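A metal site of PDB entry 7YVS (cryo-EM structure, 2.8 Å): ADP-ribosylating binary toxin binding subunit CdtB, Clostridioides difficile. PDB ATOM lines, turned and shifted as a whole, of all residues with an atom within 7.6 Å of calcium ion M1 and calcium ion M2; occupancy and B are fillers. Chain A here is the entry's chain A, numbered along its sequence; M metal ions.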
ATOM      1  N   LEU A  18     -14.191 -30.340  -0.771  1.00  0.00           N
ATOM      2  CA  LEU A  18     -14.754 -31.310  -1.706  1.00  0.00           C
ATOM      3  C   LEU A  18     -15.313 -30.571  -2.921  1.00  0.00           C
ATOM      4  O   LEU A  18     -16.123 -29.647  -2.767  1.00  0.00           O
ATOM      5  CB  LEU A  18     -15.854 -32.131  -1.030  1.00  0.00           C
ATOM      6  CG  LEU A  18     -16.531 -33.228  -1.837  1.00  0.00           C
ATOM      7  CD1 LEU A  18     -15.525 -34.262  -2.298  1.00  0.00           C
ATOM      8  CD2 LEU A  18     -17.607 -33.885  -0.997  1.00  0.00           C
ATOM      9  N   ASP A  19     -14.877 -30.975  -4.112  1.00  0.00           N
ATOM     10  CA  ASP A  19     -15.231 -30.300  -5.363  1.00  0.00           C
ATOM     11  C   ASP A  19     -15.779 -31.347  -6.319  1.00  0.00           C
ATOM     12  O   ASP A  19     -15.009 -32.018  -7.019  1.00  0.00           O
ATOM     13  CB  ASP A  19     -14.028 -29.580  -5.937  1.00  0.00           C
ATOM     14  CG  ASP A  19     -14.400 -28.520  -6.933  1.00  0.00           C
ATOM     15  OD1 ASP A  19     -15.613 -28.301  -7.138  1.00  0.00           O
ATOM     16  OD2 ASP A  19     -13.494 -27.898  -7.515  1.00  0.00           O
ATOM     17  N   THR A  20     -17.097 -31.484  -6.365  1.00  0.00           N
ATOM     18  CA  THR A  20     -17.722 -32.532  -7.175  1.00  0.00           C
ATOM     19  C   THR A  20     -17.627 -32.212  -8.670  1.00  0.00           C
ATOM     20  O   THR A  20     -17.303 -33.090  -9.475  1.00  0.00           O
ATOM     21  CB  THR A  20     -19.174 -32.728  -6.760  1.00  0.00           C
ATOM     22  OG1 THR A  20     -19.238 -32.926  -5.335  1.00  0.00           O
ATOM     23  CG2 THR A  20     -19.772 -33.939  -7.446  1.00  0.00           C
ATOM     24  N   ASP A  21     -17.917 -30.972  -9.048  1.00  0.00           N
ATOM     25  CA  ASP A  21     -17.940 -30.620 -10.461  1.00  0.00           C
ATOM     26  C   ASP A  21     -16.595 -30.166 -11.003  1.00  0.00           C
ATOM     27  O   ASP A  21     -16.489 -29.914 -12.205  1.00  0.00           O
ATOM     28  CB  ASP A  21     -18.981 -29.519 -10.717  1.00  0.00           C
ATOM     29  CG  ASP A  21     -18.894 -28.408  -9.709  1.00  0.00           C
ATOM     30  OD1 ASP A  21     -18.091 -28.525  -8.768  1.00  0.00           O
ATOM     31  OD2 ASP A  21     -19.635 -27.418  -9.863  1.00  0.00           O
ATOM     32  N   ASN A  22     -15.584 -30.045 -10.146  1.00  0.00           N
ATOM     33  CA  ASN A  22     -14.231 -29.654 -10.548  1.00  0.00           C
ATOM     34  C   ASN A  22     -14.214 -28.279 -11.216  1.00  0.00           C
ATOM     35  O   ASN A  22     -13.823 -28.119 -12.372  1.00  0.00           O
ATOM     36  CB  ASN A  22     -13.615 -30.718 -11.473  1.00  0.00           C
ATOM     37  CG  ASN A  22     -13.293 -32.005 -10.752  1.00  0.00           C
ATOM     38  OD1 ASN A  22     -12.521 -32.021  -9.801  1.00  0.00           O
ATOM     39  ND2 ASN A  22     -13.885 -33.100 -11.219  1.00  0.00           N
ATOM     40  N   ASP A  23     -14.647 -27.269 -10.449  1.00  0.00           N
ATOM     41  CA  ASP A  23     -14.545 -25.882 -10.898  1.00  0.00           C
ATOM     42  C   ASP A  23     -13.821 -25.015  -9.876  1.00  0.00           C
ATOM     43  O   ASP A  23     -14.071 -23.807  -9.821  1.00  0.00           O
ATOM     44  CB  ASP A  23     -15.924 -25.305 -11.208  1.00  0.00           C
ATOM     45  CG  ASP A  23     -16.882 -25.421 -10.044  1.00  0.00           C
ATOM     46  OD1 ASP A  23     -16.544 -26.094  -9.052  1.00  0.00           O
ATOM     47  OD2 ASP A  23     -17.978 -24.831 -10.135  1.00  0.00           O
ATOM     48  N   ASN A  24     -12.957 -25.604  -9.048  1.00  0.00           N
ATOM     49  CA  ASN A  24     -12.117 -24.893  -8.095  1.00  0.00           C
ATOM     50  C   ASN A  24     -12.921 -24.227  -6.980  1.00  0.00           C
ATOM     51  O   ASN A  24     -12.376 -23.398  -6.241  1.00  0.00           O
ATOM     52  CB  ASN A  24     -11.238 -23.856  -8.789  1.00  0.00           C
ATOM     53  CG  ASN A  24     -10.382 -24.456  -9.882  1.00  0.00           C
ATOM     54  OD1 ASN A  24     -10.355 -25.674 -10.071  1.00  0.00           O
ATOM     55  ND2 ASN A  24      -9.681 -23.607 -10.618  1.00  0.00           N
ATOM     56  N   ILE A  25     -14.191 -24.571  -6.830  1.00  0.00           N
ATOM     57  CA  ILE A  25     -14.998 -24.045  -5.728  1.00  0.00           C
ATOM     58  C   ILE A  25     -15.542 -25.215  -4.931  1.00  0.00           C
ATOM     59  O   ILE A  25     -16.196 -26.098  -5.499  1.00  0.00           O
ATOM     60  CB  ILE A  25     -16.132 -23.142  -6.233  1.00  0.00           C
ATOM     61  CG1 ILE A  25     -15.633 -22.197  -7.318  1.00  0.00           C
ATOM     62  CG2 ILE A  25     -16.702 -22.328  -5.096  1.00  0.00           C
ATOM     63  CD1 ILE A  25     -16.732 -21.482  -8.050  1.00  0.00           C
ATOM     64  N   PRO A  26     -15.298 -25.276  -3.619  1.00  0.00           N
ATOM     65  CA  PRO A  26     -15.813 -26.396  -2.825  1.00  0.00           C
ATOM     66  C   PRO A  26     -17.330 -26.416  -2.794  1.00  0.00           C
ATOM     67  O   PRO A  26     -17.987 -25.393  -2.979  1.00  0.00           O
ATOM     68  CB  PRO A  26     -15.224 -26.141  -1.432  1.00  0.00           C
ATOM     69  CG  PRO A  26     -14.054 -25.252  -1.672  1.00  0.00           C
ATOM     70  CD  PRO A  26     -14.425 -24.399  -2.828  1.00  0.00           C
ATOM     71  N   ASP A  27     -17.879 -27.607  -2.553  1.00  0.00           N
ATOM     72  CA  ASP A  27     -19.321 -27.782  -2.583  1.00  0.00           C
ATOM     73  C   ASP A  27     -20.019 -26.927  -1.537  1.00  0.00           C
ATOM     74  O   ASP A  27     -21.038 -26.288  -1.820  1.00  0.00           O
ATOM     75  CB  ASP A  27     -19.673 -29.259  -2.384  1.00  0.00           C
ATOM     76  CG  ASP A  27     -19.300 -30.107  -3.571  1.00  0.00           C
ATOM     77  OD1 ASP A  27     -18.863 -29.543  -4.598  1.00  0.00           O
ATOM     78  OD2 ASP A  27     -19.438 -31.341  -3.490  1.00  0.00           O
ATOM     79  N   SER A  28     -19.489 -26.895  -0.314  1.00  0.00           N
ATOM     80  CA  SER A  28     -20.125 -26.126   0.744  1.00  0.00           C
ATOM     81  C   SER A  28     -20.066 -24.636   0.478  1.00  0.00           C
ATOM     82  O   SER A  28     -21.006 -23.909   0.820  1.00  0.00           O
ATOM     83  CB  SER A  28     -19.484 -26.455   2.097  1.00  0.00           C
ATOM     84  OG  SER A  28     -18.083 -26.248   2.062  1.00  0.00           O
ATOM     85  N   GLU A  30     -20.143 -23.172  -2.520  1.00  0.00           N
ATOM     86  CA  GLU A  30     -21.197 -22.916  -3.501  1.00  0.00           C
ATOM     87  C   GLU A  30     -22.571 -22.981  -2.852  1.00  0.00           C
ATOM     88  O   GLU A  30     -23.473 -22.207  -3.185  1.00  0.00           O
ATOM     89  CB  GLU A  30     -21.117 -23.920  -4.642  1.00  0.00           C
ATOM     90  CG  GLU A  30     -19.850 -23.878  -5.435  1.00  0.00           C
ATOM     91  CD  GLU A  30     -20.003 -24.525  -6.783  1.00  0.00           C
ATOM     92  OE1 GLU A  30     -20.786 -24.012  -7.605  1.00  0.00           O
ATOM     93  OE2 GLU A  30     -19.341 -25.548  -7.033  1.00  0.00           O
ATOM     94  N   TYR A  34     -20.041 -17.557  -1.221  1.00  0.00           N
ATOM     95  CA  TYR A  34     -18.601 -17.357  -1.341  1.00  0.00           C
ATOM     96  C   TYR A  34     -18.334 -16.061  -2.091  1.00  0.00           C
ATOM     97  O   TYR A  34     -19.249 -15.403  -2.583  1.00  0.00           O
ATOM     98  CB  TYR A  34     -17.928 -18.537  -2.069  1.00  0.00           C
ATOM     99  CG  TYR A  34     -18.405 -18.743  -3.481  1.00  0.00           C
ATOM    100  CD1 TYR A  34     -19.564 -19.450  -3.746  1.00  0.00           C
ATOM    101  CD2 TYR A  34     -17.695 -18.243  -4.563  1.00  0.00           C
ATOM    102  CE1 TYR A  34     -20.010 -19.646  -5.037  1.00  0.00           C
ATOM    103  CE2 TYR A  34     -18.127 -18.432  -5.848  1.00  0.00           C
ATOM    104  CZ  TYR A  34     -19.283 -19.134  -6.080  1.00  0.00           C
ATOM    105  OH  TYR A  34     -19.725 -19.332  -7.362  1.00  0.00           O
ATOM    106  N   SER A  58     -24.167 -20.890  -6.300  1.00  0.00           N
ATOM    107  CA  SER A  58     -24.207 -21.561  -7.593  1.00  0.00           C
ATOM    108  C   SER A  58     -24.515 -23.040  -7.391  1.00  0.00           C
ATOM    109  O   SER A  58     -24.669 -23.511  -6.263  1.00  0.00           O
ATOM    110  CB  SER A  58     -22.894 -21.375  -8.347  1.00  0.00           C
ATOM    111  OG  SER A  58     -21.798 -21.878  -7.608  1.00  0.00           O
ATOM    112  N   ASN A  59     -24.604 -23.748  -8.502  1.00  0.00           N
ATOM    113  CA  ASN A  59     -24.905 -25.175  -8.505  1.00  0.00           C
ATOM    114  C   ASN A  59     -23.624 -25.955  -8.232  1.00  0.00           C
ATOM    115  O   ASN A  59     -22.651 -25.828  -8.967  1.00  0.00           O
ATOM    116  CB  ASN A  59     -25.516 -25.570  -9.836  1.00  0.00           C
ATOM    117  CG  ASN A  59     -26.138 -26.945  -9.819  1.00  0.00           C
ATOM    118  OD1 ASN A  59     -25.892 -27.741  -8.918  1.00  0.00           O
ATOM    119  ND2 ASN A  59     -26.955 -27.234 -10.816  1.00  0.00           N
ATOM    120  N   TYR A  60     -23.628 -26.774  -7.180  1.00  0.00           N
ATOM    121  CA  TYR A  60     -22.444 -27.533  -6.826  1.00  0.00           C
ATOM    122  C   TYR A  60     -22.321 -28.830  -7.618  1.00  0.00           C
ATOM    123  O   TYR A  60     -21.324 -29.542  -7.438  1.00  0.00           O
ATOM    124  CB  TYR A  60     -22.407 -27.818  -5.329  1.00  0.00           C
ATOM    125  CG  TYR A  60     -23.355 -28.890  -4.843  1.00  0.00           C
ATOM    126  CD1 TYR A  60     -24.687 -28.601  -4.572  1.00  0.00           C
ATOM    127  CD2 TYR A  60     -22.923 -30.189  -4.641  1.00  0.00           C
ATOM    128  CE1 TYR A  60     -25.544 -29.579  -4.122  1.00  0.00           C
ATOM    129  CE2 TYR A  60     -23.770 -31.167  -4.195  1.00  0.00           C
ATOM    130  CZ  TYR A  60     -25.087 -30.857  -3.937  1.00  0.00           C
ATOM    131  OH  TYR A  60     -25.944 -31.835  -3.487  1.00  0.00           O
ATOM    132  N   LEU A  61     -23.288 -29.147  -8.464  1.00  0.00           N
ATOM    133  CA  LEU A  61     -23.227 -30.316  -9.337  1.00  0.00           C
ATOM    134  C   LEU A  61     -23.032 -29.935 -10.799  1.00  0.00           C
ATOM    135  O   LEU A  61     -22.864 -30.830 -11.637  1.00  0.00           O
ATOM    136  CB  LEU A  61     -24.487 -31.159  -9.171  1.00  0.00           C
ATOM    137  CG  LEU A  61     -24.533 -32.049  -7.923  1.00  0.00           C
ATOM    138  CD1 LEU A  61     -25.816 -32.841  -7.881  1.00  0.00           C
ATOM    139  CD2 LEU A  61     -23.340 -32.971  -7.881  1.00  0.00           C
ATOM    140  N   GLU A  62     -23.047 -28.644 -11.124  1.00  0.00           N
ATOM    141  CA  GLU A  62     -22.815 -28.152 -12.471  1.00  0.00           C
ATOM    142  C   GLU A  62     -21.612 -27.223 -12.463  1.00  0.00           C
ATOM    143  O   GLU A  62     -21.475 -26.378 -11.582  1.00  0.00           O
ATOM    144  CB  GLU A  62     -24.028 -27.402 -13.013  1.00  0.00           C
ATOM    145  CG  GLU A  62     -25.103 -28.295 -13.594  1.00  0.00           C
ATOM    146  CD  GLU A  62     -24.716 -28.886 -14.930  1.00  0.00           C
ATOM    147  OE1 GLU A  62     -23.885 -28.261 -15.633  1.00  0.00           O
ATOM    148  OE2 GLU A  62     -25.223 -29.973 -15.279  1.00  0.00           O
ATOM    149  N   SER A  63     -20.737 -27.383 -13.462  1.00  0.00           N
ATOM    150  CA  SER A  63     -19.606 -26.485 -13.617  1.00  0.00           C
ATOM    151  C   SER A  63     -20.005 -25.189 -14.313  1.00  0.00           C
ATOM    152  O   SER A  63     -19.286 -24.193 -14.209  1.00  0.00           O
ATOM    153  CB  SER A  63     -18.480 -27.172 -14.379  1.00  0.00           C
ATOM    154  OG  SER A  63     -17.283 -26.444 -14.250  1.00  0.00           O
ATOM    155  N   ASN A  64     -21.114 -25.194 -15.039  1.00  0.00           N
ATOM    156  CA  ASN A  64     -21.659 -24.008 -15.700  1.00  0.00           C
ATOM    157  C   ASN A  64     -23.118 -23.894 -15.259  1.00  0.00           C
ATOM    158  O   ASN A  64     -24.005 -24.472 -15.889  1.00  0.00           O
ATOM    159  CB  ASN A  64     -21.526 -24.104 -17.210  1.00  0.00           C
ATOM    160  CG  ASN A  64     -20.097 -24.223 -17.672  1.00  0.00           C
ATOM    161  OD1 ASN A  64     -19.366 -25.107 -17.238  1.00  0.00           O
ATOM    162  ND2 ASN A  64     -19.689 -23.345 -18.573  1.00  0.00           N
ATOM    163  N   THR A  65     -23.362 -23.145 -14.181  1.00  0.00           N
ATOM    164  CA  THR A  65     -24.706 -23.064 -13.630  1.00  0.00           C
ATOM    165  C   THR A  65     -25.668 -22.378 -14.596  1.00  0.00           C
ATOM    166  O   THR A  65     -26.822 -22.801 -14.734  1.00  0.00           O
ATOM    167  CB  THR A  65     -24.673 -22.318 -12.298  1.00  0.00           C
ATOM    168  OG1 THR A  65     -23.724 -22.957 -11.429  1.00  0.00           O
ATOM    169  CG2 THR A  65     -26.032 -22.335 -11.637  1.00  0.00           C
ATOM    170  N   THR A  71     -17.378 -21.073 -17.017  1.00  0.00           N
ATOM    171  CA  THR A  71     -17.649 -21.817 -15.798  1.00  0.00           C
ATOM    172  C   THR A  71     -17.988 -20.862 -14.651  1.00  0.00           C
ATOM    173  O   THR A  71     -17.876 -19.642 -14.767  1.00  0.00           O
ATOM    174  CB  THR A  71     -16.445 -22.684 -15.407  1.00  0.00           C
ATOM    175  OG1 THR A  71     -15.452 -21.874 -14.793  1.00  0.00           O
ATOM    176  CG2 THR A  71     -15.860 -23.354 -16.624  1.00  0.00           C
ATOM    177  N   ASP A  72     -18.430 -21.440 -13.536  1.00  0.00           N
ATOM    178  CA  ASP A  72     -18.784 -20.617 -12.383  1.00  0.00           C
ATOM    179  C   ASP A  72     -17.584 -19.854 -11.849  1.00  0.00           C
ATOM    180  O   ASP A  72     -17.690 -18.676 -11.520  1.00  0.00           O
ATOM    181  CB  ASP A  72     -19.393 -21.497 -11.293  1.00  0.00           C
ATOM    182  CG  ASP A  72     -20.729 -22.092 -11.703  1.00  0.00           C
ATOM    183  OD1 ASP A  72     -21.332 -21.595 -12.664  1.00  0.00           O
ATOM    184  OD2 ASP A  72     -21.167 -23.061 -11.049  1.00  0.00           O
ATOM    185  N   TYR A  73     -16.434 -20.517 -11.763  1.00  0.00           N
ATOM    186  CA  TYR A  73     -15.223 -19.848 -11.284  1.00  0.00           C
ATOM    187  C   TYR A  73     -14.779 -18.759 -12.239  1.00  0.00           C
ATOM    188  O   TYR A  73     -14.396 -17.670 -11.802  1.00  0.00           O
ATOM    189  CB  TYR A  73     -14.099 -20.853 -11.082  1.00  0.00           C
ATOM    190  CG  TYR A  73     -12.794 -20.199 -10.714  1.00  0.00           C
ATOM    191  CD1 TYR A  73     -12.561 -19.716  -9.442  1.00  0.00           C
ATOM    192  CD2 TYR A  73     -11.785 -20.050 -11.661  1.00  0.00           C
ATOM    193  CE1 TYR A  73     -11.370 -19.113  -9.110  1.00  0.00           C
ATOM    194  CE2 TYR A  73     -10.597 -19.445 -11.338  1.00  0.00           C
ATOM    195  CZ  TYR A  73     -10.397 -18.980 -10.066  1.00  0.00           C
ATOM    196  OH  TYR A  73      -9.210 -18.375  -9.744  1.00  0.00           O
ATOM    197  N   PRO A  91     -22.682 -16.260 -11.054  1.00  0.00           N
ATOM    198  CA  PRO A  91     -22.968 -17.513 -11.754  1.00  0.00           C
ATOM    199  C   PRO A  91     -24.414 -17.679 -12.214  1.00  0.00           C
ATOM    200  O   PRO A  91     -24.666 -18.486 -13.103  1.00  0.00           O
ATOM    201  CB  PRO A  91     -22.602 -18.578 -10.723  1.00  0.00           C
ATOM    202  CG  PRO A  91     -21.623 -17.915  -9.830  1.00  0.00           C
ATOM    203  CD  PRO A  91     -22.067 -16.502  -9.730  1.00  0.00           C
HETATM  204 CA    CA M   1     -17.609 -27.064  -7.096  1.00  0.00          CA
HETATM  205 CA    CA M   2     -20.483 -25.156  -9.760  1.00  0.00          CA
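The backbone carbonyl oxygen of Glu 30 is in hydrogen-bond range of the backbone NH of Ser 58, at 3.5 Å. The side-chain carboxylate (OD2) of Asp 19 lies within hydrogen-bond range of the backbone NH (N) of Asn 24 (2.8 Å). The side-chain hydroxyl (OG1) of Thr 65 is in hydrogen-bond range of the backbone NH (N) of Asn 59 (3.2 Å). The backbone NH of Leu 61 is in hydrogen-bond range of the side-chain amide oxygen of Asn 59. The backbone NH (N) of Asp 72 lies within hydrogen-bond range of the backbone carbonyl oxygen (O) of Ser 63 (3.0 Å). The side-chain carboxylate (OD1) of Asp 72 lies within hydrogen-bond range of the backbone NH (N) of Thr 65 (3.0 Å). OD2 of Asp 27 sits at hydrogen-bond distance from OG1 of Thr 20, 2.4 Å away. N of Asp 27 sits at hydrogen-bond distance from O of Leu 18, at 2.7 Å.
Residues that only touch calcium ion M1: Asp 27 (3.7 Å). Of the 25 residues printed, 6 come within 4 Å of calcium ion M1.
Calcium ion M1 is bound by OD1 of Asp 21 (2.3 Å), OE2 of Glu 30 (2.3 Å), O of Ile 25 (2.3 Å), OD1 of Asp 19 (2.3 Å) and OD1 of Asp 23 (2.4 Å).
Calcium ion M2 is bound by O of Asn 59, O of Glu 62, OD2 of Asp 21, OE1 of Glu 30, OD2 of Asp 72 and OD2 of Asp 23. Slightly farther from calcium ion M2 lies the side-chain carboxylate (OE2) of Glu 30 (3.0 Å).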
